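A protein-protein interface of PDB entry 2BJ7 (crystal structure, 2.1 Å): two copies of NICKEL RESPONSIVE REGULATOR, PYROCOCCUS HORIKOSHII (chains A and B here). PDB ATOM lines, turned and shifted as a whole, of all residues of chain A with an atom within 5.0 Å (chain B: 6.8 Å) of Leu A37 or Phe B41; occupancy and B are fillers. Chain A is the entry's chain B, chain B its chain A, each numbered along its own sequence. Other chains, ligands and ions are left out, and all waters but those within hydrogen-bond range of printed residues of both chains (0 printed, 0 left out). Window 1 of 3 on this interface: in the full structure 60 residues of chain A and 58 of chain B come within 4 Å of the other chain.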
ATOM      1  N   PHE A  18      16.311  37.628  25.107  1.00  0.00           N
ATOM      2  CA  PHE A  18      15.567  36.581  24.412  1.00  0.00           C
ATOM      3  C   PHE A  18      14.908  37.121  23.136  1.00  0.00           C
ATOM      4  O   PHE A  18      15.080  36.552  22.050  1.00  0.00           O
ATOM      5  CB  PHE A  18      14.500  36.009  25.348  1.00  0.00           C
ATOM      6  CG  PHE A  18      13.751  34.832  24.782  1.00  0.00           C
ATOM      7  CD1 PHE A  18      14.427  33.674  24.408  1.00  0.00           C
ATOM      8  CD2 PHE A  18      12.361  34.869  24.661  1.00  0.00           C
ATOM      9  CE1 PHE A  18      13.730  32.565  23.927  1.00  0.00           C
ATOM     10  CE2 PHE A  18      11.654  33.764  24.180  1.00  0.00           C
ATOM     11  CZ  PHE A  18      12.339  32.611  23.814  1.00  0.00           C
ATOM     12  N   ILE A  21      17.470  37.782  20.378  1.00  0.00           N
ATOM     13  CA  ILE A  21      17.950  36.564  19.740  1.00  0.00           C
ATOM     14  C   ILE A  21      16.924  35.877  18.838  1.00  0.00           C
ATOM     15  O   ILE A  21      17.217  35.583  17.679  1.00  0.00           O
ATOM     16  CB  ILE A  21      18.442  35.549  20.796  1.00  0.00           C
ATOM     17  CG1 ILE A  21      19.679  36.107  21.501  1.00  0.00           C
ATOM     18  CG2 ILE A  21      18.776  34.215  20.140  1.00  0.00           C
ATOM     19  CD1 ILE A  21      20.217  35.206  22.593  1.00  0.00           C
ATOM     20  N   ILE A  22      15.721  35.627  19.344  1.00  0.00           N
ATOM     21  CA  ILE A  22      14.744  34.935  18.513  1.00  0.00           C
ATOM     22  C   ILE A  22      14.427  35.686  17.230  1.00  0.00           C
ATOM     23  O   ILE A  22      14.087  35.076  16.214  1.00  0.00           O
ATOM     24  CB  ILE A  22      13.442  34.633  19.272  1.00  0.00           C
ATOM     25  CG1 ILE A  22      12.683  35.918  19.571  1.00  0.00           C
ATOM     26  CG2 ILE A  22      13.764  33.861  20.549  1.00  0.00           C
ATOM     27  CD1 ILE A  22      11.390  35.665  20.303  1.00  0.00           C
ATOM     28  N   ILE A  25      17.283  34.895  14.886  1.00  0.00           N
ATOM     29  CA  ILE A  25      17.186  33.513  14.426  1.00  0.00           C
ATOM     30  C   ILE A  25      16.161  33.367  13.307  1.00  0.00           C
ATOM     31  O   ILE A  25      16.376  32.619  12.352  1.00  0.00           O
ATOM     32  CB  ILE A  25      16.780  32.557  15.572  1.00  0.00           C
ATOM     33  CG1 ILE A  25      17.931  32.407  16.563  1.00  0.00           C
ATOM     34  CG2 ILE A  25      16.404  31.192  15.006  1.00  0.00           C
ATOM     35  CD1 ILE A  25      17.597  31.507  17.738  1.00  0.00           C
ATOM     36  N   TYR A  27      12.468  33.597  14.255  1.00  0.00           N
ATOM     37  CA  TYR A  27      11.144  33.382  14.835  1.00  0.00           C
ATOM     38  C   TYR A  27      10.274  34.610  14.589  1.00  0.00           C
ATOM     39  O   TYR A  27      10.746  35.743  14.672  1.00  0.00           O
ATOM     40  CB  TYR A  27      11.226  33.154  16.343  1.00  0.00           C
ATOM     41  CG  TYR A  27      11.559  31.744  16.746  1.00  0.00           C
ATOM     42  CD1 TYR A  27      12.853  31.395  17.124  1.00  0.00           C
ATOM     43  CD2 TYR A  27      10.576  30.755  16.757  1.00  0.00           C
ATOM     44  CE1 TYR A  27      13.162  30.099  17.510  1.00  0.00           C
ATOM     45  CE2 TYR A  27      10.873  29.453  17.138  1.00  0.00           C
ATOM     46  CZ  TYR A  27      12.170  29.135  17.515  1.00  0.00           C
ATOM     47  OH  TYR A  27      12.477  27.851  17.899  1.00  0.00           O
ATOM     48  N   ALA A  33       8.502  30.865  19.941  1.00  0.00           N
ATOM     49  CA  ALA A  33       9.777  30.420  20.482  1.00  0.00           C
ATOM     50  C   ALA A  33       9.594  29.741  21.834  1.00  0.00           C
ATOM     51  O   ALA A  33      10.213  28.714  22.109  1.00  0.00           O
ATOM     52  CB  ALA A  33      10.736  31.603  20.608  1.00  0.00           C
ATOM     53  N   ILE A  34       8.738  30.302  22.676  1.00  0.00           N
ATOM     54  CA  ILE A  34       8.502  29.716  23.986  1.00  0.00           C
ATOM     55  C   ILE A  34       7.794  28.365  23.870  1.00  0.00           C
ATOM     56  O   ILE A  34       8.109  27.430  24.617  1.00  0.00           O
ATOM     57  CB  ILE A  34       7.701  30.680  24.890  1.00  0.00           C
ATOM     58  CG1 ILE A  34       8.537  31.937  25.150  1.00  0.00           C
ATOM     59  CG2 ILE A  34       7.350  29.995  26.211  1.00  0.00           C
ATOM     60  CD1 ILE A  34       7.855  32.985  26.004  1.00  0.00           C
ATOM     61  N   ARG A  35       6.847  28.244  22.941  1.00  0.00           N
ATOM     62  CA  ARG A  35       6.171  26.960  22.770  1.00  0.00           C
ATOM     63  C   ARG A  35       7.207  25.934  22.307  1.00  0.00           C
ATOM     64  O   ARG A  35       7.141  24.763  22.687  1.00  0.00           O
ATOM     65  CB  ARG A  35       5.015  27.060  21.763  1.00  0.00           C
ATOM     66  CG  ARG A  35       3.733  27.665  22.357  1.00  0.00           C
ATOM     67  CD  ARG A  35       2.512  27.454  21.445  1.00  0.00           C
ATOM     68  NE  ARG A  35       2.570  28.291  20.255  1.00  0.00           N
ATOM     69  CZ  ARG A  35       2.277  29.588  20.238  1.00  0.00           C
ATOM     70  NH1 ARG A  35       2.374  30.273  19.109  1.00  0.00           N
ATOM     71  NH2 ARG A  35       1.869  30.197  21.346  1.00  0.00           N
ATOM     72  N   ASP A  36       8.168  26.372  21.492  1.00  0.00           N
ATOM     73  CA  ASP A  36       9.223  25.472  21.030  1.00  0.00           C
ATOM     74  C   ASP A  36      10.077  25.051  22.233  1.00  0.00           C
ATOM     75  O   ASP A  36      10.459  23.891  22.351  1.00  0.00           O
ATOM     76  CB  ASP A  36      10.109  26.153  19.976  1.00  0.00           C
ATOM     77  CG  ASP A  36       9.736  25.767  18.545  1.00  0.00           C
ATOM     78  OD1 ASP A  36      10.358  26.310  17.601  1.00  0.00           O
ATOM     79  OD2 ASP A  36       8.827  24.920  18.362  1.00  0.00           O
ATOM     80  N   LEU A  37      10.365  25.991  23.130  1.00  0.00           N
ATOM     81  CA  LEU A  37      11.160  25.673  24.313  1.00  0.00           C
ATOM     82  C   LEU A  37      10.452  24.610  25.137  1.00  0.00           C
ATOM     83  O   LEU A  37      11.083  23.687  25.651  1.00  0.00           O
ATOM     84  CB  LEU A  37      11.384  26.916  25.182  1.00  0.00           C
ATOM     85  CG  LEU A  37      12.250  28.028  24.584  1.00  0.00           C
ATOM     86  CD1 LEU A  37      12.473  29.116  25.627  1.00  0.00           C
ATOM     87  CD2 LEU A  37      13.582  27.455  24.124  1.00  0.00           C
ATOM     88  N   ILE A  38       9.138  24.746  25.263  1.00  0.00           N
ATOM     89  CA  ILE A  38       8.350  23.797  26.034  1.00  0.00           C
ATOM     90  C   ILE A  38       8.314  22.419  25.365  1.00  0.00           C
ATOM     91  O   ILE A  38       8.375  21.392  26.046  1.00  0.00           O
ATOM     92  CB  ILE A  38       6.917  24.353  26.268  1.00  0.00           C
ATOM     93  CG1 ILE A  38       7.009  25.546  27.234  1.00  0.00           C
ATOM     94  CG2 ILE A  38       5.992  23.265  26.827  1.00  0.00           C
ATOM     95  CD1 ILE A  38       5.699  26.297  27.452  1.00  0.00           C
ATOM     96  N   ARG A  39       8.212  22.392  24.040  1.00  0.00           N
ATOM     97  CA  ARG A  39       8.214  21.119  23.328  1.00  0.00           C
ATOM     98  C   ARG A  39       9.569  20.439  23.536  1.00  0.00           C
ATOM     99  O   ARG A  39       9.648  19.228  23.780  1.00  0.00           O
ATOM    100  CB  ARG A  39       7.976  21.332  21.829  1.00  0.00           C
ATOM    101  CG  ARG A  39       6.511  21.404  21.423  1.00  0.00           C
ATOM    102  CD  ARG A  39       6.382  21.434  19.902  1.00  0.00           C
ATOM    103  NE  ARG A  39       6.687  22.753  19.360  1.00  0.00           N
ATOM    104  CZ  ARG A  39       5.767  23.691  19.151  1.00  0.00           C
ATOM    105  NH1 ARG A  39       4.496  23.436  19.431  1.00  0.00           N
ATOM    106  NH2 ARG A  39       6.118  24.883  18.686  1.00  0.00           N
ATOM    107  N   ASP A  40      10.635  21.229  23.450  1.00  0.00           N
ATOM    108  CA  ASP A  40      11.977  20.702  23.623  1.00  0.00           C
ATOM    109  C   ASP A  40      12.137  20.126  25.027  1.00  0.00           C
ATOM    110  O   ASP A  40      12.719  19.058  25.213  1.00  0.00           O
ATOM    111  CB  ASP A  40      13.008  21.806  23.401  1.00  0.00           C
ATOM    112  CG  ASP A  40      14.435  21.330  23.665  1.00  0.00           C
ATOM    113  OD1 ASP A  40      14.902  20.428  22.939  1.00  0.00           O
ATOM    114  OD2 ASP A  40      15.086  21.850  24.600  1.00  0.00           O
ATOM    115  N   PHE A  41      11.613  20.844  26.013  1.00  0.00           N
ATOM    116  CA  PHE A  41      11.688  20.417  27.406  1.00  0.00           C
ATOM    117  C   PHE A  41      10.947  19.095  27.617  1.00  0.00           C
ATOM    118  O   PHE A  41      11.434  18.207  28.321  1.00  0.00           O
ATOM    119  CB  PHE A  41      11.108  21.522  28.299  1.00  0.00           C
ATOM    120  CG  PHE A  41      11.091  21.190  29.767  1.00  0.00           C
ATOM    121  CD1 PHE A  41       9.912  20.795  30.389  1.00  0.00           C
ATOM    122  CD2 PHE A  41      12.244  21.321  30.538  1.00  0.00           C
ATOM    123  CE1 PHE A  41       9.876  20.541  31.767  1.00  0.00           C
ATOM    124  CE2 PHE A  41      12.223  21.069  31.909  1.00  0.00           C
ATOM    125  CZ  PHE A  41      11.034  20.679  32.526  1.00  0.00           C
ATOM    126  N   PHE B  18       3.501  19.779  30.365  1.00  0.00           N
ATOM    127  CA  PHE B  18       4.496  20.688  30.907  1.00  0.00           C
ATOM    128  C   PHE B  18       4.275  20.869  32.398  1.00  0.00           C
ATOM    129  O   PHE B  18       5.230  20.841  33.176  1.00  0.00           O
ATOM    130  CB  PHE B  18       4.421  22.047  30.200  1.00  0.00           C
ATOM    131  CG  PHE B  18       5.431  23.047  30.691  1.00  0.00           C
ATOM    132  CD1 PHE B  18       6.791  22.860  30.454  1.00  0.00           C
ATOM    133  CD2 PHE B  18       5.021  24.194  31.371  1.00  0.00           C
ATOM    134  CE1 PHE B  18       7.735  23.807  30.885  1.00  0.00           C
ATOM    135  CE2 PHE B  18       5.953  25.148  31.805  1.00  0.00           C
ATOM    136  CZ  PHE B  18       7.313  24.956  31.563  1.00  0.00           C
ATOM    137  N   ILE B  34      10.015  28.362  32.785  1.00  0.00           N
ATOM    138  CA  ILE B  34      10.211  29.028  31.507  1.00  0.00           C
ATOM    139  C   ILE B  34      11.414  29.957  31.558  1.00  0.00           C
ATOM    140  O   ILE B  34      12.162  30.084  30.581  1.00  0.00           O
ATOM    141  CB  ILE B  34       8.922  29.765  31.089  1.00  0.00           C
ATOM    142  CG1 ILE B  34       7.826  28.724  30.843  1.00  0.00           C
ATOM    143  CG2 ILE B  34       9.163  30.598  29.835  1.00  0.00           C
ATOM    144  CD1 ILE B  34       6.432  29.297  30.706  1.00  0.00           C
ATOM    145  N   ASP B  36      14.068  29.447  33.193  1.00  0.00           N
ATOM    146  CA  ASP B  36      15.247  28.602  33.030  1.00  0.00           C
ATOM    147  C   ASP B  36      15.418  28.150  31.585  1.00  0.00           C
ATOM    148  O   ASP B  36      16.540  28.118  31.062  1.00  0.00           O
ATOM    149  CB  ASP B  36      15.178  27.398  33.974  1.00  0.00           C
ATOM    150  CG  ASP B  36      15.342  27.799  35.437  1.00  0.00           C
ATOM    151  OD1 ASP B  36      15.881  28.903  35.690  1.00  0.00           O
ATOM    152  OD2 ASP B  36      14.948  27.017  36.332  1.00  0.00           O
ATOM    153  N   LEU B  37      14.306  27.820  30.932  1.00  0.00           N
ATOM    154  CA  LEU B  37      14.355  27.393  29.537  1.00  0.00           C
ATOM    155  C   LEU B  37      14.886  28.528  28.666  1.00  0.00           C
ATOM    156  O   LEU B  37      15.658  28.299  27.737  1.00  0.00           O
ATOM    157  CB  LEU B  37      12.964  26.983  29.060  1.00  0.00           C
ATOM    158  CG  LEU B  37      12.360  25.772  29.774  1.00  0.00           C
ATOM    159  CD1 LEU B  37      10.989  25.460  29.193  1.00  0.00           C
ATOM    160  CD2 LEU B  37      13.299  24.576  29.621  1.00  0.00           C
ATOM    161  N   ILE B  38      14.477  29.755  28.971  1.00  0.00           N
ATOM    162  CA  ILE B  38      14.931  30.907  28.193  1.00  0.00           C
ATOM    163  C   ILE B  38      16.420  31.172  28.399  1.00  0.00           C
ATOM    164  O   ILE B  38      17.141  31.471  27.444  1.00  0.00           O
ATOM    165  CB  ILE B  38      14.112  32.187  28.558  1.00  0.00           C
ATOM    166  CG1 ILE B  38      12.687  32.055  28.007  1.00  0.00           C
ATOM    167  CG2 ILE B  38      14.783  33.430  28.004  1.00  0.00           C
ATOM    168  CD1 ILE B  38      11.762  33.210  28.362  1.00  0.00           C
ATOM    169  N   ARG B  39      16.887  31.069  29.639  1.00  0.00           N
ATOM    170  CA  ARG B  39      18.300  31.312  29.915  1.00  0.00           C
ATOM    171  C   ARG B  39      19.179  30.297  29.189  1.00  0.00           C
ATOM    172  O   ARG B  39      20.189  30.660  28.582  1.00  0.00           O
ATOM    173  CB  ARG B  39      18.591  31.234  31.412  1.00  0.00           C
ATOM    174  CG  ARG B  39      20.024  31.657  31.761  1.00  0.00           C
ATOM    175  CD  ARG B  39      20.422  31.236  33.169  1.00  0.00           C
ATOM    176  NE  ARG B  39      19.365  31.497  34.143  1.00  0.00           N
ATOM    177  CZ  ARG B  39      18.647  30.550  34.741  1.00  0.00           C
ATOM    178  NH1 ARG B  39      18.873  29.267  34.469  1.00  0.00           N
ATOM    179  NH2 ARG B  39      17.701  30.884  35.610  1.00  0.00           N
ATOM    180  N   ASP B  40      18.791  29.025  29.257  1.00  0.00           N
ATOM    181  CA  ASP B  40      19.551  27.962  28.603  1.00  0.00           C
ATOM    182  C   ASP B  40      19.581  28.193  27.111  1.00  0.00           C
ATOM    183  O   ASP B  40      20.611  28.018  26.460  1.00  0.00           O
ATOM    184  CB  ASP B  40      18.923  26.599  28.900  1.00  0.00           C
ATOM    185  CG  ASP B  40      19.050  26.211  30.358  1.00  0.00           C
ATOM    186  OD1 ASP B  40      18.364  25.259  30.789  1.00  0.00           O
ATOM    187  OD2 ASP B  40      19.847  26.855  31.076  1.00  0.00           O
ATOM    188  N   PHE B  41      18.437  28.594  26.571  1.00  0.00           N
ATOM    189  CA  PHE B  41      18.320  28.860  25.149  1.00  0.00           C
ATOM    190  C   PHE B  41      19.305  29.942  24.725  1.00  0.00           C
ATOM    191  O   PHE B  41      20.021  29.793  23.735  1.00  0.00           O
ATOM    192  CB  PHE B  41      16.898  29.310  24.821  1.00  0.00           C
ATOM    193  CG  PHE B  41      16.685  29.616  23.371  1.00  0.00           C
ATOM    194  CD1 PHE B  41      16.409  28.597  22.466  1.00  0.00           C
ATOM    195  CD2 PHE B  41      16.755  30.927  22.910  1.00  0.00           C
ATOM    196  CE1 PHE B  41      16.203  28.880  21.117  1.00  0.00           C
ATOM    197  CE2 PHE B  41      16.553  31.219  21.566  1.00  0.00           C
ATOM    198  CZ  PHE B  41      16.274  30.194  20.668  1.00  0.00           C
ATOM    199  N   ILE B  42      19.330  31.041  25.471  1.00  0.00           N
ATOM    200  CA  ILE B  42      20.236  32.140  25.153  1.00  0.00           C
ATOM    201  C   ILE B  42      21.688  31.664  25.173  1.00  0.00           C
ATOM    202  O   ILE B  42      22.471  31.958  24.265  1.00  0.00           O
ATOM    203  CB  ILE B  42      20.072  33.292  26.160  1.00  0.00           C
ATOM    204  CG1 ILE B  42      18.681  33.923  25.996  1.00  0.00           C
ATOM    205  CG2 ILE B  42      21.176  34.324  25.950  1.00  0.00           C
ATOM    206  CD1 ILE B  42      18.370  35.016  26.994  1.00  0.00           C
ATOM    207  N   ILE B  43      22.039  30.924  26.217  1.00  0.00           N
ATOM    208  CA  ILE B  43      23.390  30.409  26.360  1.00  0.00           C
ATOM    209  C   ILE B  43      23.789  29.536  25.167  1.00  0.00           C
ATOM    210  O   ILE B  43      24.870  29.714  24.603  1.00  0.00           O
ATOM    211  CB  ILE B  43      23.526  29.616  27.682  1.00  0.00           C
ATOM    212  CG1 ILE B  43      23.419  30.591  28.862  1.00  0.00           C
ATOM    213  CG2 ILE B  43      24.850  28.857  27.712  1.00  0.00           C
ATOM    214  CD1 ILE B  43      23.427  29.939  30.230  1.00  0.00           C
ATOM    215  N   ARG B  44      22.914  28.617  24.767  1.00  0.00           N
ATOM    216  CA  ARG B  44      23.206  27.743  23.636  1.00  0.00           C
ATOM    217  C   ARG B  44      23.291  28.508  22.322  1.00  0.00           C
ATOM    218  O   ARG B  44      24.002  28.101  21.408  1.00  0.00           O
ATOM    219  CB  ARG B  44      22.146  26.646  23.497  1.00  0.00           C
ATOM    220  CG  ARG B  44      22.040  25.699  24.680  1.00  0.00           C
ATOM    221  CD  ARG B  44      21.235  24.460  24.293  1.00  0.00           C
ATOM    222  NE  ARG B  44      19.892  24.788  23.809  1.00  0.00           N
ATOM    223  CZ  ARG B  44      18.856  25.067  24.596  1.00  0.00           C
ATOM    224  NH1 ARG B  44      18.999  25.059  25.915  1.00  0.00           N
ATOM    225  NH2 ARG B  44      17.675  25.354  24.066  1.00  0.00           N
ATOM    226  N   HIS B  45      22.568  29.616  22.223  1.00  0.00           N
ATOM    227  CA  HIS B  45      22.575  30.403  20.999  1.00  0.00           C
ATOM    228  C   HIS B  45      23.561  31.555  21.003  1.00  0.00           C
ATOM    229  O   HIS B  45      23.517  32.417  20.129  1.00  0.00           O
ATOM    230  CB  HIS B  45      21.171  30.924  20.714  1.00  0.00           C
ATOM    231  CG  HIS B  45      20.233  29.863  20.242  1.00  0.00           C
ATOM    232  ND1 HIS B  45      20.069  29.556  18.908  1.00  0.00           N
ATOM    233  CD2 HIS B  45      19.454  28.994  20.928  1.00  0.00           C
ATOM    234  CE1 HIS B  45      19.230  28.543  18.794  1.00  0.00           C
ATOM    235  NE2 HIS B  45      18.843  28.182  20.004  1.00  0.00           N
ATOM    236  N   GLU B  46      24.452  31.576  21.986  1.00  0.00           N
ATOM    237  CA  GLU B  46      25.450  32.633  22.056  1.00  0.00           C
ATOM    238  C   GLU B  46      26.849  32.113  21.747  1.00  0.00           C
ATOM    239  O   GLU B  46      27.728  32.885  21.366  1.00  0.00           O
ATOM    240  CB  GLU B  46      25.413  33.315  23.425  1.00  0.00           C
ATOM    241  CG  GLU B  46      24.417  34.470  23.481  1.00  0.00           C
ATOM    242  CD  GLU B  46      24.351  35.135  24.843  1.00  0.00           C
ATOM    243  OE1 GLU B  46      23.760  36.234  24.936  1.00  0.00           O
ATOM    244  OE2 GLU B  46      24.882  34.556  25.817  1.00  0.00           O
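Printed residues of chain B that touch a printed residue of chain A: Phe B18, Leu B37, Ile B38, Phe B41, Ile B42 and His B45.
Hydrophobic or aromatic side chains of chain B that line the printed part of chain A: Phe B18, Leu B37, Ile B38, Phe B41, Ile B42 and His B45.
Among the printed residues, no Asp or Glu carboxylate lies within 4 Å of a Lys or Arg side-chain nitrogen of the other chain.
The backbone NH (N) of Tyr A27 sits at hydrogen-bond distance from the backbone carbonyl oxygen (O) of Ile A22.
Printed residues of chain B within 4 Å of Ile A21: Phe B41 (3.99 Å) and Ile B42 (3.6 Å).
Of the printed residues of chain B, Ile A25 touches Phe B41 and His B45.
Ile A34 touches none of the printed residues of chain B.
Of chain B, only Leu B37 (3.9 Å), Ile B38 (3.8 Å) and Phe B41 (3.5 Å) come within 4 Å of Leu A37.
Of the printed residues of chain A, Phe B18 touches Ile A38 and Phe A41.
Asp B40 touches none of the printed residues of chain A.
Of the printed residues of chain A, Ile B42 touches Phe A18 (3.8 Å) and Ile A21 (3.6 Å).
The nearest printed residue of chain A that does not touch Phe B18 is Leu A37 (6.2 Å).
Among the printed residues, pairs that only touch across the chains: Ile A25 with His B45 (3.4 Å), Leu A37 with Phe B41 (3.5 Å), Ile A25 with Phe B41 (3.5 Å), Phe A41 with Leu B37 (3.5 Å), Phe A18 with Phe B41 (3.6 Å), Ile A21 with Ile B42 (3.6 Å), Phe A18 with Ile B38 (3.6 Å), Ile A38 with Phe B18 (3.7 Å), Phe A41 with Phe B18 (3.7 Å), Leu A37 with Ile B38 (3.8 Å), Phe A18 with Ile B42 (3.8 Å), Leu A37 with Leu B37 (3.9 Å), Ile A22 with Phe B41 (3.97 Å) and Ile A21 with Phe B41 (3.99 Å).
Phe A18 touches Ile B38, and with the chains exchanged Ile A38 touches Phe B18.
Phe A18 touches Phe B41, and with the chains exchanged Phe A41 touches Phe B18.
Leu B37 touches its own counterpart, Leu A37.
Leu A37 touches Phe B41, and with the chains exchanged Phe A41 touches Leu B37.
Of the 14 pairs that touch across the chains among the printed residues, 7 have their exchanged pair printed and touching as well.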
